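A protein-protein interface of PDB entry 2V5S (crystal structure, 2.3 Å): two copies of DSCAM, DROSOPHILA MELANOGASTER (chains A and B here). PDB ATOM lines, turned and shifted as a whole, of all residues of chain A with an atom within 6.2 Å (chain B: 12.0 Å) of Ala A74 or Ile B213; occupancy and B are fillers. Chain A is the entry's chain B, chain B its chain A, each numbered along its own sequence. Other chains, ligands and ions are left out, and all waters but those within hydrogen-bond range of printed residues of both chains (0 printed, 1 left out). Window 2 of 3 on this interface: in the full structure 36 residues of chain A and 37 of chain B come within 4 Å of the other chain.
No residue of chain B comes within 4 Å of Phe A72. Of chain B, only Ile B213 comes within 4 Å of Ala A74. Asp A76 touches none of the printed residues of chain B. Of chain B, only Ile B213, Ser B214 and Ser B215 come within 4 Å of Tyr A77. No residue of chain B comes within 4 Å of Ala A109. Of the printed residues of chain B, Gln A110 touches Thr B210 (3.0 Å), Glu B211 (2.3 Å), Pro B212 (3.7 Å) and Ile B213 (3.8 Å). Of the printed residues of chain A, Thr B210 touches Gln A110 (3.0 Å). Of the printed residues of chain A, Glu B211 touches Gln A110. Printed residues of chain A within 4 Å of Pro B212: Gln A110. Of chain A, only Ala A74, Tyr A77 and Gln A110 come within 4 Å of Ile B213. The nearest residue of chain B that does not touch Ala A74 is Ser B214 (6.7 Å). The nearest residue of chain A that does not touch Ile B213 is Val A108 (4.04 Å). The nearest printed residue of chain B that does not touch Gln A110 is Ser B214 (6.1 Å).
No position is printed for both chains.
O of Val B121 lies within hydrogen-bond range of N of Thr B210 (2.8 Å). The backbone NH of Arg B123 sits at hydrogen-bond distance from the backbone carbonyl oxygen of Thr B210. The guanidinium group of Arg B123 is in salt-bridge range of the side-chain carboxylate of Glu B211 (3.3 Å).
Of the 21 printed residues of chain B, 6 touch a printed residue of chain A. Of the 10 printed residues of chain A, 4 touch a printed residue of chain B. Along chain A the printed residues that touch a printed residue of chain B span positions 74 to 110. Among the printed residues, 9 pairs touch across the chains.
Among the printed residues, pairs that only touch across the chains: Gln A110 with Thr B210, Ala A74 with Ile B213, Tyr A77 with Ile B213, Gln A110 with Pro B212, Gln A110 with Ile B213 and Tyr A77 with Ser B214.
The side-chain hydroxyl (OG) of Ser B214 lies within hydrogen-bond range of the backbone NH (N) of Val A108 (2.8 Å). N of Ser B215 is in hydrogen-bond range of OH of Tyr A77 (3.1 Å). NE2 of Gln A110 sits close to O of Glu B211 (2.3 Å).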
ATOM      1  N   ASN A  24     -10.276  -9.172 -18.629  1.00  0.00           N
ATOM      2  CA  ASN A  24     -10.018  -7.813 -19.106  1.00  0.00           C
ATOM      3  C   ASN A  24     -11.120  -6.830 -18.752  1.00  0.00           C
ATOM      4  O   ASN A  24     -10.883  -5.633 -18.660  1.00  0.00           O
ATOM      5  CB  ASN A  24      -9.766  -7.758 -20.612  1.00  0.00           C
ATOM      6  CG  ASN A  24     -10.976  -8.144 -21.437  1.00  0.00           C
ATOM      7  OD1 ASN A  24     -11.369  -9.307 -21.447  1.00  0.00           O
ATOM      8  ND2 ASN A  24     -11.521  -7.172 -22.183  1.00  0.00           N
ATOM      9  N   PHE A  72      -9.646  -3.195 -19.427  1.00  0.00           N
ATOM     10  CA  PHE A  72      -9.024  -2.712 -20.655  1.00  0.00           C
ATOM     11  C   PHE A  72      -9.553  -3.416 -21.912  1.00  0.00           C
ATOM     12  O   PHE A  72     -10.130  -4.500 -21.840  1.00  0.00           O
ATOM     13  CB  PHE A  72      -7.505  -2.888 -20.532  1.00  0.00           C
ATOM     14  CG  PHE A  72      -7.078  -4.328 -20.413  1.00  0.00           C
ATOM     15  CD1 PHE A  72      -6.631  -5.039 -21.508  1.00  0.00           C
ATOM     16  CD2 PHE A  72      -7.164  -4.987 -19.203  1.00  0.00           C
ATOM     17  CE1 PHE A  72      -6.301  -6.378 -21.401  1.00  0.00           C
ATOM     18  CE2 PHE A  72      -6.776  -6.282 -19.047  1.00  0.00           C
ATOM     19  CZ  PHE A  72      -6.354  -6.995 -20.157  1.00  0.00           C
ATOM     20  N   ARG A  73      -9.351  -2.789 -23.066  1.00  0.00           N
ATOM     21  CA  ARG A  73      -9.771  -3.313 -24.365  1.00  0.00           C
ATOM     22  C   ARG A  73      -8.805  -4.372 -24.913  1.00  0.00           C
ATOM     23  O   ARG A  73      -7.591  -4.298 -24.739  1.00  0.00           O
ATOM     24  CB  ARG A  73      -9.913  -2.162 -25.373  1.00  0.00           C
ATOM     25  CG  ARG A  73     -10.533  -0.872 -24.816  1.00  0.00           C
ATOM     26  CD  ARG A  73     -11.166   0.099 -25.822  1.00  0.00           C
ATOM     27  NE  ARG A  73     -11.624   1.334 -25.178  1.00  0.00           N
ATOM     28  CZ  ARG A  73     -12.546   2.182 -25.639  1.00  0.00           C
ATOM     29  NH1 ARG A  73     -13.191   1.984 -26.787  1.00  0.00           N
ATOM     30  NH2 ARG A  73     -12.845   3.259 -24.920  1.00  0.00           N
ATOM     31  N   ALA A  74      -9.329  -5.363 -25.627  1.00  0.00           N
ATOM     32  CA  ALA A  74      -8.518  -6.447 -26.190  1.00  0.00           C
ATOM     33  C   ALA A  74      -7.250  -5.949 -26.885  1.00  0.00           C
ATOM     34  O   ALA A  74      -6.172  -6.505 -26.716  1.00  0.00           O
ATOM     35  CB  ALA A  74      -9.360  -7.255 -27.168  1.00  0.00           C
ATOM     36  N   GLU A  75      -7.423  -4.875 -27.648  1.00  0.00           N
ATOM     37  CA  GLU A  75      -6.413  -4.207 -28.451  1.00  0.00           C
ATOM     38  C   GLU A  75      -5.278  -3.782 -27.529  1.00  0.00           C
ATOM     39  O   GLU A  75      -4.183  -3.517 -28.024  1.00  0.00           O
ATOM     40  CB  GLU A  75      -7.041  -2.965 -29.111  1.00  0.00           C
ATOM     41  CG  GLU A  75      -8.095  -3.133 -30.228  1.00  0.00           C
ATOM     42  CD  GLU A  75      -9.333  -3.987 -29.934  1.00  0.00           C
ATOM     43  OE1 GLU A  75     -10.110  -3.699 -28.998  1.00  0.00           O
ATOM     44  OE2 GLU A  75      -9.579  -4.961 -30.683  1.00  0.00           O
ATOM     45  N   ASP A  76      -5.547  -3.659 -26.231  1.00  0.00           N
ATOM     46  CA  ASP A  76      -4.615  -3.021 -25.304  1.00  0.00           C
ATOM     47  C   ASP A  76      -3.847  -4.040 -24.460  1.00  0.00           C
ATOM     48  O   ASP A  76      -3.151  -3.677 -23.518  1.00  0.00           O
ATOM     49  CB  ASP A  76      -5.341  -2.044 -24.365  1.00  0.00           C
ATOM     50  CG  ASP A  76      -5.759  -0.720 -25.018  1.00  0.00           C
ATOM     51  OD1 ASP A  76      -5.319  -0.386 -26.144  1.00  0.00           O
ATOM     52  OD2 ASP A  76      -6.560   0.004 -24.380  1.00  0.00           O
ATOM     53  N   TYR A  77      -3.956  -5.329 -24.758  1.00  0.00           N
ATOM     54  CA  TYR A  77      -3.298  -6.361 -23.948  1.00  0.00           C
ATOM     55  C   TYR A  77      -1.812  -6.162 -24.137  1.00  0.00           C
ATOM     56  O   TYR A  77      -1.389  -5.930 -25.266  1.00  0.00           O
ATOM     57  CB  TYR A  77      -3.662  -7.760 -24.430  1.00  0.00           C
ATOM     58  CG  TYR A  77      -2.956  -8.873 -23.701  1.00  0.00           C
ATOM     59  CD1 TYR A  77      -3.478  -9.388 -22.516  1.00  0.00           C
ATOM     60  CD2 TYR A  77      -1.795  -9.436 -24.212  1.00  0.00           C
ATOM     61  CE1 TYR A  77      -2.831 -10.413 -21.855  1.00  0.00           C
ATOM     62  CE2 TYR A  77      -1.131 -10.418 -23.524  1.00  0.00           C
ATOM     63  CZ  TYR A  77      -1.660 -10.911 -22.365  1.00  0.00           C
ATOM     64  OH  TYR A  77      -1.021 -11.941 -21.719  1.00  0.00           O
ATOM     65  N   VAL A 108      -8.232 -11.971 -21.733  1.00  0.00           N
ATOM     66  CA  VAL A 108      -9.243 -11.388 -22.598  1.00  0.00           C
ATOM     67  C   VAL A 108     -10.346 -12.388 -22.908  1.00  0.00           C
ATOM     68  O   VAL A 108     -10.098 -13.528 -23.314  1.00  0.00           O
ATOM     69  CB  VAL A 108      -8.647 -10.793 -23.877  1.00  0.00           C
ATOM     70  CG1 VAL A 108      -9.780 -10.248 -24.762  1.00  0.00           C
ATOM     71  CG2 VAL A 108      -7.611  -9.662 -23.576  1.00  0.00           C
ATOM     72  N   ALA A 109     -11.574 -11.954 -22.637  1.00  0.00           N
ATOM     73  CA  ALA A 109     -12.805 -12.714 -22.906  1.00  0.00           C
ATOM     74  C   ALA A 109     -12.842 -13.284 -24.319  1.00  0.00           C
ATOM     75  O   ALA A 109     -12.965 -12.499 -25.274  1.00  0.00           O
ATOM     76  CB  ALA A 109     -14.047 -11.821 -22.681  1.00  0.00           C
ATOM     77  N   GLN A 110     -12.711 -14.606 -24.429  1.00  0.00           N
ATOM     78  CA  GLN A 110     -12.786 -15.263 -25.727  1.00  0.00           C
ATOM     79  C   GLN A 110     -13.734 -16.459 -25.776  1.00  0.00           C
ATOM     80  O   GLN A 110     -13.846 -17.221 -24.818  1.00  0.00           O
ATOM     81  CB  GLN A 110     -11.426 -15.786 -26.163  1.00  0.00           C
ATOM     82  CG  GLN A 110     -10.639 -14.977 -27.183  1.00  0.00           C
ATOM     83  CD  GLN A 110      -9.675 -15.857 -27.978  1.00  0.00           C
ATOM     84  OE1 GLN A 110      -9.234 -16.918 -27.521  1.00  0.00           O
ATOM     85  NE2 GLN A 110      -9.416 -15.457 -29.214  1.00  0.00           N
ATOM     86  N   VAL B 121      -7.012 -25.966 -31.314  1.00  0.00           N
ATOM     87  CA  VAL B 121      -5.634 -25.536 -31.290  1.00  0.00           C
ATOM     88  C   VAL B 121      -5.519 -24.039 -31.496  1.00  0.00           C
ATOM     89  O   VAL B 121      -6.341 -23.382 -32.114  1.00  0.00           O
ATOM     90  CB  VAL B 121      -4.822 -26.316 -32.362  1.00  0.00           C
ATOM     91  CG1 VAL B 121      -5.006 -27.808 -32.125  1.00  0.00           C
ATOM     92  CG2 VAL B 121      -5.285 -25.944 -33.765  1.00  0.00           C
ATOM     93  N   ILE B 122      -4.440 -23.499 -30.955  1.00  0.00           N
ATOM     94  CA  ILE B 122      -4.104 -22.080 -31.012  1.00  0.00           C
ATOM     95  C   ILE B 122      -3.320 -21.897 -32.308  1.00  0.00           C
ATOM     96  O   ILE B 122      -2.370 -22.640 -32.524  1.00  0.00           O
ATOM     97  CB  ILE B 122      -3.198 -21.703 -29.817  1.00  0.00           C
ATOM     98  CG1 ILE B 122      -3.943 -21.895 -28.487  1.00  0.00           C
ATOM     99  CG2 ILE B 122      -2.770 -20.227 -29.880  1.00  0.00           C
ATOM    100  CD1 ILE B 122      -3.265 -21.285 -27.261  1.00  0.00           C
ATOM    101  N   ARG B 123      -3.738 -20.974 -33.165  1.00  0.00           N
ATOM    102  CA  ARG B 123      -3.037 -20.587 -34.379  1.00  0.00           C
ATOM    103  C   ARG B 123      -1.542 -20.538 -34.149  1.00  0.00           C
ATOM    104  O   ARG B 123      -1.039 -19.925 -33.204  1.00  0.00           O
ATOM    105  CB  ARG B 123      -3.519 -19.222 -34.849  1.00  0.00           C
ATOM    106  CG  ARG B 123      -3.018 -18.834 -36.222  1.00  0.00           C
ATOM    107  CD  ARG B 123      -3.269 -17.359 -36.450  1.00  0.00           C
ATOM    108  NE  ARG B 123      -2.737 -16.914 -37.734  1.00  0.00           N
ATOM    109  CZ  ARG B 123      -3.273 -15.964 -38.495  1.00  0.00           C
ATOM    110  NH1 ARG B 123      -4.380 -15.326 -38.138  1.00  0.00           N
ATOM    111  NH2 ARG B 123      -2.684 -15.645 -39.635  1.00  0.00           N
ATOM    112  N   GLY B 124      -0.828 -21.286 -34.979  1.00  0.00           N
ATOM    113  CA  GLY B 124       0.635 -21.252 -34.989  1.00  0.00           C
ATOM    114  C   GLY B 124       1.289 -22.397 -34.245  1.00  0.00           C
ATOM    115  O   GLY B 124       2.504 -22.575 -34.314  1.00  0.00           O
ATOM    116  N   ASN B 125       0.481 -23.122 -33.476  1.00  0.00           N
ATOM    117  CA  ASN B 125       0.938 -24.327 -32.804  1.00  0.00           C
ATOM    118  C   ASN B 125       0.858 -25.510 -33.788  1.00  0.00           C
ATOM    119  O   ASN B 125       0.101 -25.483 -34.772  1.00  0.00           O
ATOM    120  CB  ASN B 125       0.081 -24.591 -31.555  1.00  0.00           C
ATOM    121  CG  ASN B 125       0.392 -23.645 -30.398  1.00  0.00           C
ATOM    122  OD1 ASN B 125       0.940 -24.054 -29.367  1.00  0.00           O
ATOM    123  ND2 ASN B 125       0.037 -22.372 -30.559  1.00  0.00           N
ATOM    124  N   ILE B 209      -9.503 -23.671 -34.847  1.00  0.00           N
ATOM    125  CA  ILE B 209      -8.379 -22.789 -34.543  1.00  0.00           C
ATOM    126  C   ILE B 209      -8.811 -21.578 -33.723  1.00  0.00           C
ATOM    127  O   ILE B 209      -9.670 -20.824 -34.173  1.00  0.00           O
ATOM    128  CB  ILE B 209      -7.731 -22.252 -35.831  1.00  0.00           C
ATOM    129  CG1 ILE B 209      -7.114 -23.369 -36.684  1.00  0.00           C
ATOM    130  CG2 ILE B 209      -6.647 -21.238 -35.495  1.00  0.00           C
ATOM    131  CD1 ILE B 209      -8.018 -24.014 -37.689  1.00  0.00           C
ATOM    132  N   THR B 210      -8.187 -21.333 -32.575  1.00  0.00           N
ATOM    133  CA  THR B 210      -8.339 -20.050 -31.901  1.00  0.00           C
ATOM    134  C   THR B 210      -7.213 -19.079 -32.213  1.00  0.00           C
ATOM    135  O   THR B 210      -6.033 -19.449 -32.251  1.00  0.00           O
ATOM    136  CB  THR B 210      -8.403 -20.205 -30.401  1.00  0.00           C
ATOM    137  OG1 THR B 210      -9.504 -21.068 -30.139  1.00  0.00           O
ATOM    138  CG2 THR B 210      -8.741 -18.925 -29.712  1.00  0.00           C
ATOM    139  N   GLU B 211      -7.657 -17.853 -32.477  1.00  0.00           N
ATOM    140  CA  GLU B 211      -6.786 -16.707 -32.654  1.00  0.00           C
ATOM    141  C   GLU B 211      -6.734 -16.079 -31.276  1.00  0.00           C
ATOM    142  O   GLU B 211      -7.698 -15.482 -30.808  1.00  0.00           O
ATOM    143  CB  GLU B 211      -7.353 -15.601 -33.554  1.00  0.00           C
ATOM    144  CG  GLU B 211      -8.340 -15.921 -34.696  1.00  0.00           C
ATOM    145  CD  GLU B 211      -7.896 -16.772 -35.875  1.00  0.00           C
ATOM    146  OE1 GLU B 211      -7.338 -16.204 -36.841  1.00  0.00           O
ATOM    147  OE2 GLU B 211      -8.247 -17.974 -35.879  1.00  0.00           O
ATOM    148  N   PRO B 212      -5.589 -16.163 -30.604  1.00  0.00           N
ATOM    149  CA  PRO B 212      -5.714 -15.777 -29.204  1.00  0.00           C
ATOM    150  C   PRO B 212      -5.357 -14.305 -29.003  1.00  0.00           C
ATOM    151  O   PRO B 212      -4.582 -13.759 -29.781  1.00  0.00           O
ATOM    152  CB  PRO B 212      -4.709 -16.719 -28.536  1.00  0.00           C
ATOM    153  CG  PRO B 212      -4.028 -17.470 -29.705  1.00  0.00           C
ATOM    154  CD  PRO B 212      -4.228 -16.621 -30.924  1.00  0.00           C
ATOM    155  N   ILE B 213      -5.928 -13.632 -28.012  1.00  0.00           N
ATOM    156  CA  ILE B 213      -5.494 -12.275 -27.743  1.00  0.00           C
ATOM    157  C   ILE B 213      -4.531 -12.215 -26.560  1.00  0.00           C
ATOM    158  O   ILE B 213      -3.543 -11.475 -26.561  1.00  0.00           O
ATOM    159  CB  ILE B 213      -6.656 -11.352 -27.357  1.00  0.00           C
ATOM    160  CG1 ILE B 213      -7.922 -11.646 -28.181  1.00  0.00           C
ATOM    161  CG2 ILE B 213      -6.119  -9.902 -27.321  1.00  0.00           C
ATOM    162  CD1 ILE B 213      -7.725 -12.077 -29.626  1.00  0.00           C
ATOM    163  N   SER B 214      -4.912 -12.941 -25.516  1.00  0.00           N
ATOM    164  CA  SER B 214      -4.092 -13.145 -24.342  1.00  0.00           C
ATOM    165  C   SER B 214      -2.989 -14.125 -24.676  1.00  0.00           C
ATOM    166  O   SER B 214      -3.175 -15.057 -25.453  1.00  0.00           O
ATOM    167  CB  SER B 214      -4.918 -13.794 -23.241  1.00  0.00           C
ATOM    168  OG  SER B 214      -5.705 -12.765 -22.698  1.00  0.00           O
ATOM    169  N   SER B 215      -1.847 -13.899 -24.043  1.00  0.00           N
ATOM    170  CA  SER B 215      -0.812 -14.906 -23.946  1.00  0.00           C
ATOM    171  C   SER B 215      -1.208 -15.952 -22.905  1.00  0.00           C
ATOM    172  O   SER B 215      -2.117 -15.813 -22.078  1.00  0.00           O
ATOM    173  CB  SER B 215       0.508 -14.231 -23.581  1.00  0.00           C
ATOM    174  OG  SER B 215       0.824 -13.198 -24.493  1.00  0.00           O
ATOM    175  N   SER B 216      -0.516 -17.073 -23.030  1.00  0.00           N
ATOM    176  CA  SER B 216      -0.791 -18.210 -22.162  1.00  0.00           C
ATOM    177  C   SER B 216       0.472 -19.059 -22.183  1.00  0.00           C
ATOM    178  O   SER B 216       1.031 -19.342 -23.234  1.00  0.00           O
ATOM    179  CB  SER B 216      -2.034 -19.013 -22.585  1.00  0.00           C
ATOM    180  OG  SER B 216      -2.014 -19.413 -23.950  1.00  0.00           O
ATOM    181  N   ALA B 217       0.933 -19.386 -20.984  1.00  0.00           N
ATOM    182  CA  ALA B 217       2.016 -20.347 -20.829  1.00  0.00           C
ATOM    183  C   ALA B 217       1.540 -21.655 -21.454  1.00  0.00           C
ATOM    184  O   ALA B 217       0.339 -21.893 -21.506  1.00  0.00           O
ATOM    185  CB  ALA B 217       2.402 -20.502 -19.372  1.00  0.00           C
ATOM    186  N   GLY B 244       0.337 -23.320 -26.514  1.00  0.00           N
ATOM    187  CA  GLY B 244       0.745 -22.105 -25.819  1.00  0.00           C
ATOM    188  C   GLY B 244       0.618 -20.944 -26.782  1.00  0.00           C
ATOM    189  O   GLY B 244       0.500 -21.121 -28.006  1.00  0.00           O
ATOM    190  N   PHE B 245       0.672 -19.759 -26.186  1.00  0.00           N
ATOM    191  CA  PHE B 245       0.782 -18.540 -26.976  1.00  0.00           C
ATOM    192  C   PHE B 245       1.653 -17.464 -26.337  1.00  0.00           C
ATOM    193  O   PHE B 245       1.315 -16.976 -25.258  1.00  0.00           O
ATOM    194  CB  PHE B 245      -0.607 -17.980 -27.273  1.00  0.00           C
ATOM    195  CG  PHE B 245      -0.575 -16.867 -28.273  1.00  0.00           C
ATOM    196  CD1 PHE B 245       0.012 -17.071 -29.521  1.00  0.00           C
ATOM    197  CD2 PHE B 245      -1.085 -15.613 -27.944  1.00  0.00           C
ATOM    198  CE1 PHE B 245       0.102 -16.037 -30.441  1.00  0.00           C
ATOM    199  CE2 PHE B 245      -1.007 -14.572 -28.857  1.00  0.00           C
ATOM    200  CZ  PHE B 245      -0.408 -14.792 -30.110  1.00  0.00           C
ATOM    201  N   PRO B 246       2.763 -17.106 -27.009  1.00  0.00           N
ATOM    202  CA  PRO B 246       3.260 -17.618 -28.292  1.00  0.00           C
ATOM    203  C   PRO B 246       3.568 -19.117 -28.439  1.00  0.00           C
ATOM    204  O   PRO B 246       3.774 -19.818 -27.436  1.00  0.00           O
ATOM    205  CB  PRO B 246       4.529 -16.795 -28.545  1.00  0.00           C
ATOM    206  CG  PRO B 246       4.841 -16.086 -27.262  1.00  0.00           C
ATOM    207  CD  PRO B 246       3.532 -15.936 -26.554  1.00  0.00           C
ATOM    208  N   ALA B 247       3.541 -19.581 -29.692  1.00  0.00           N
ATOM    209  CA  ALA B 247       3.731 -20.990 -30.022  1.00  0.00           C
ATOM    210  C   ALA B 247       5.062 -21.384 -29.401  1.00  0.00           C
ATOM    211  O   ALA B 247       6.047 -20.674 -29.566  1.00  0.00           O
ATOM    212  CB  ALA B 247       3.759 -21.223 -31.522  1.00  0.00           C
ATOM    213  N   ASN B 297       7.563 -20.966 -23.457  1.00  0.00           N
ATOM    214  CA  ASN B 297       7.536 -19.697 -24.167  1.00  0.00           C
ATOM    215  C   ASN B 297       7.737 -18.541 -23.201  1.00  0.00           C
ATOM    216  O   ASN B 297       8.063 -18.749 -22.030  1.00  0.00           O
ATOM    217  CB  ASN B 297       6.237 -19.548 -24.954  1.00  0.00           C
ATOM    218  CG  ASN B 297       5.039 -19.455 -24.045  1.00  0.00           C
ATOM    219  OD1 ASN B 297       5.184 -19.322 -22.833  1.00  0.00           O
ATOM    220  ND2 ASN B 297       3.857 -19.564 -24.627  1.00  0.00           N
ATOM    221  N   SER B 298       7.591 -17.335 -23.736  1.00  0.00           N
ATOM    222  CA  SER B 298       8.013 -16.173 -22.996  1.00  0.00           C
ATOM    223  C   SER B 298       7.152 -15.960 -21.767  1.00  0.00           C
ATOM    224  O   SER B 298       7.555 -15.140 -20.950  1.00  0.00           O
ATOM    225  CB  SER B 298       8.064 -14.926 -23.876  1.00  0.00           C
ATOM    226  OG  SER B 298       6.801 -14.609 -24.417  1.00  0.00           O
ATOM    227  N   VAL B 299       6.029 -16.669 -21.649  1.00  0.00           N
ATOM    228  CA  VAL B 299       5.202 -16.583 -20.447  1.00  0.00           C
ATOM    229  C   VAL B 299       5.655 -17.629 -19.420  1.00  0.00           C
ATOM    230  O   VAL B 299       5.718 -17.337 -18.233  1.00  0.00           O
ATOM    231  CB  VAL B 299       3.695 -16.789 -20.728  1.00  0.00           C
ATOM    232  CG1 VAL B 299       2.880 -16.446 -19.468  1.00  0.00           C
ATOM    233  CG2 VAL B 299       3.198 -15.960 -21.901  1.00  0.00           C
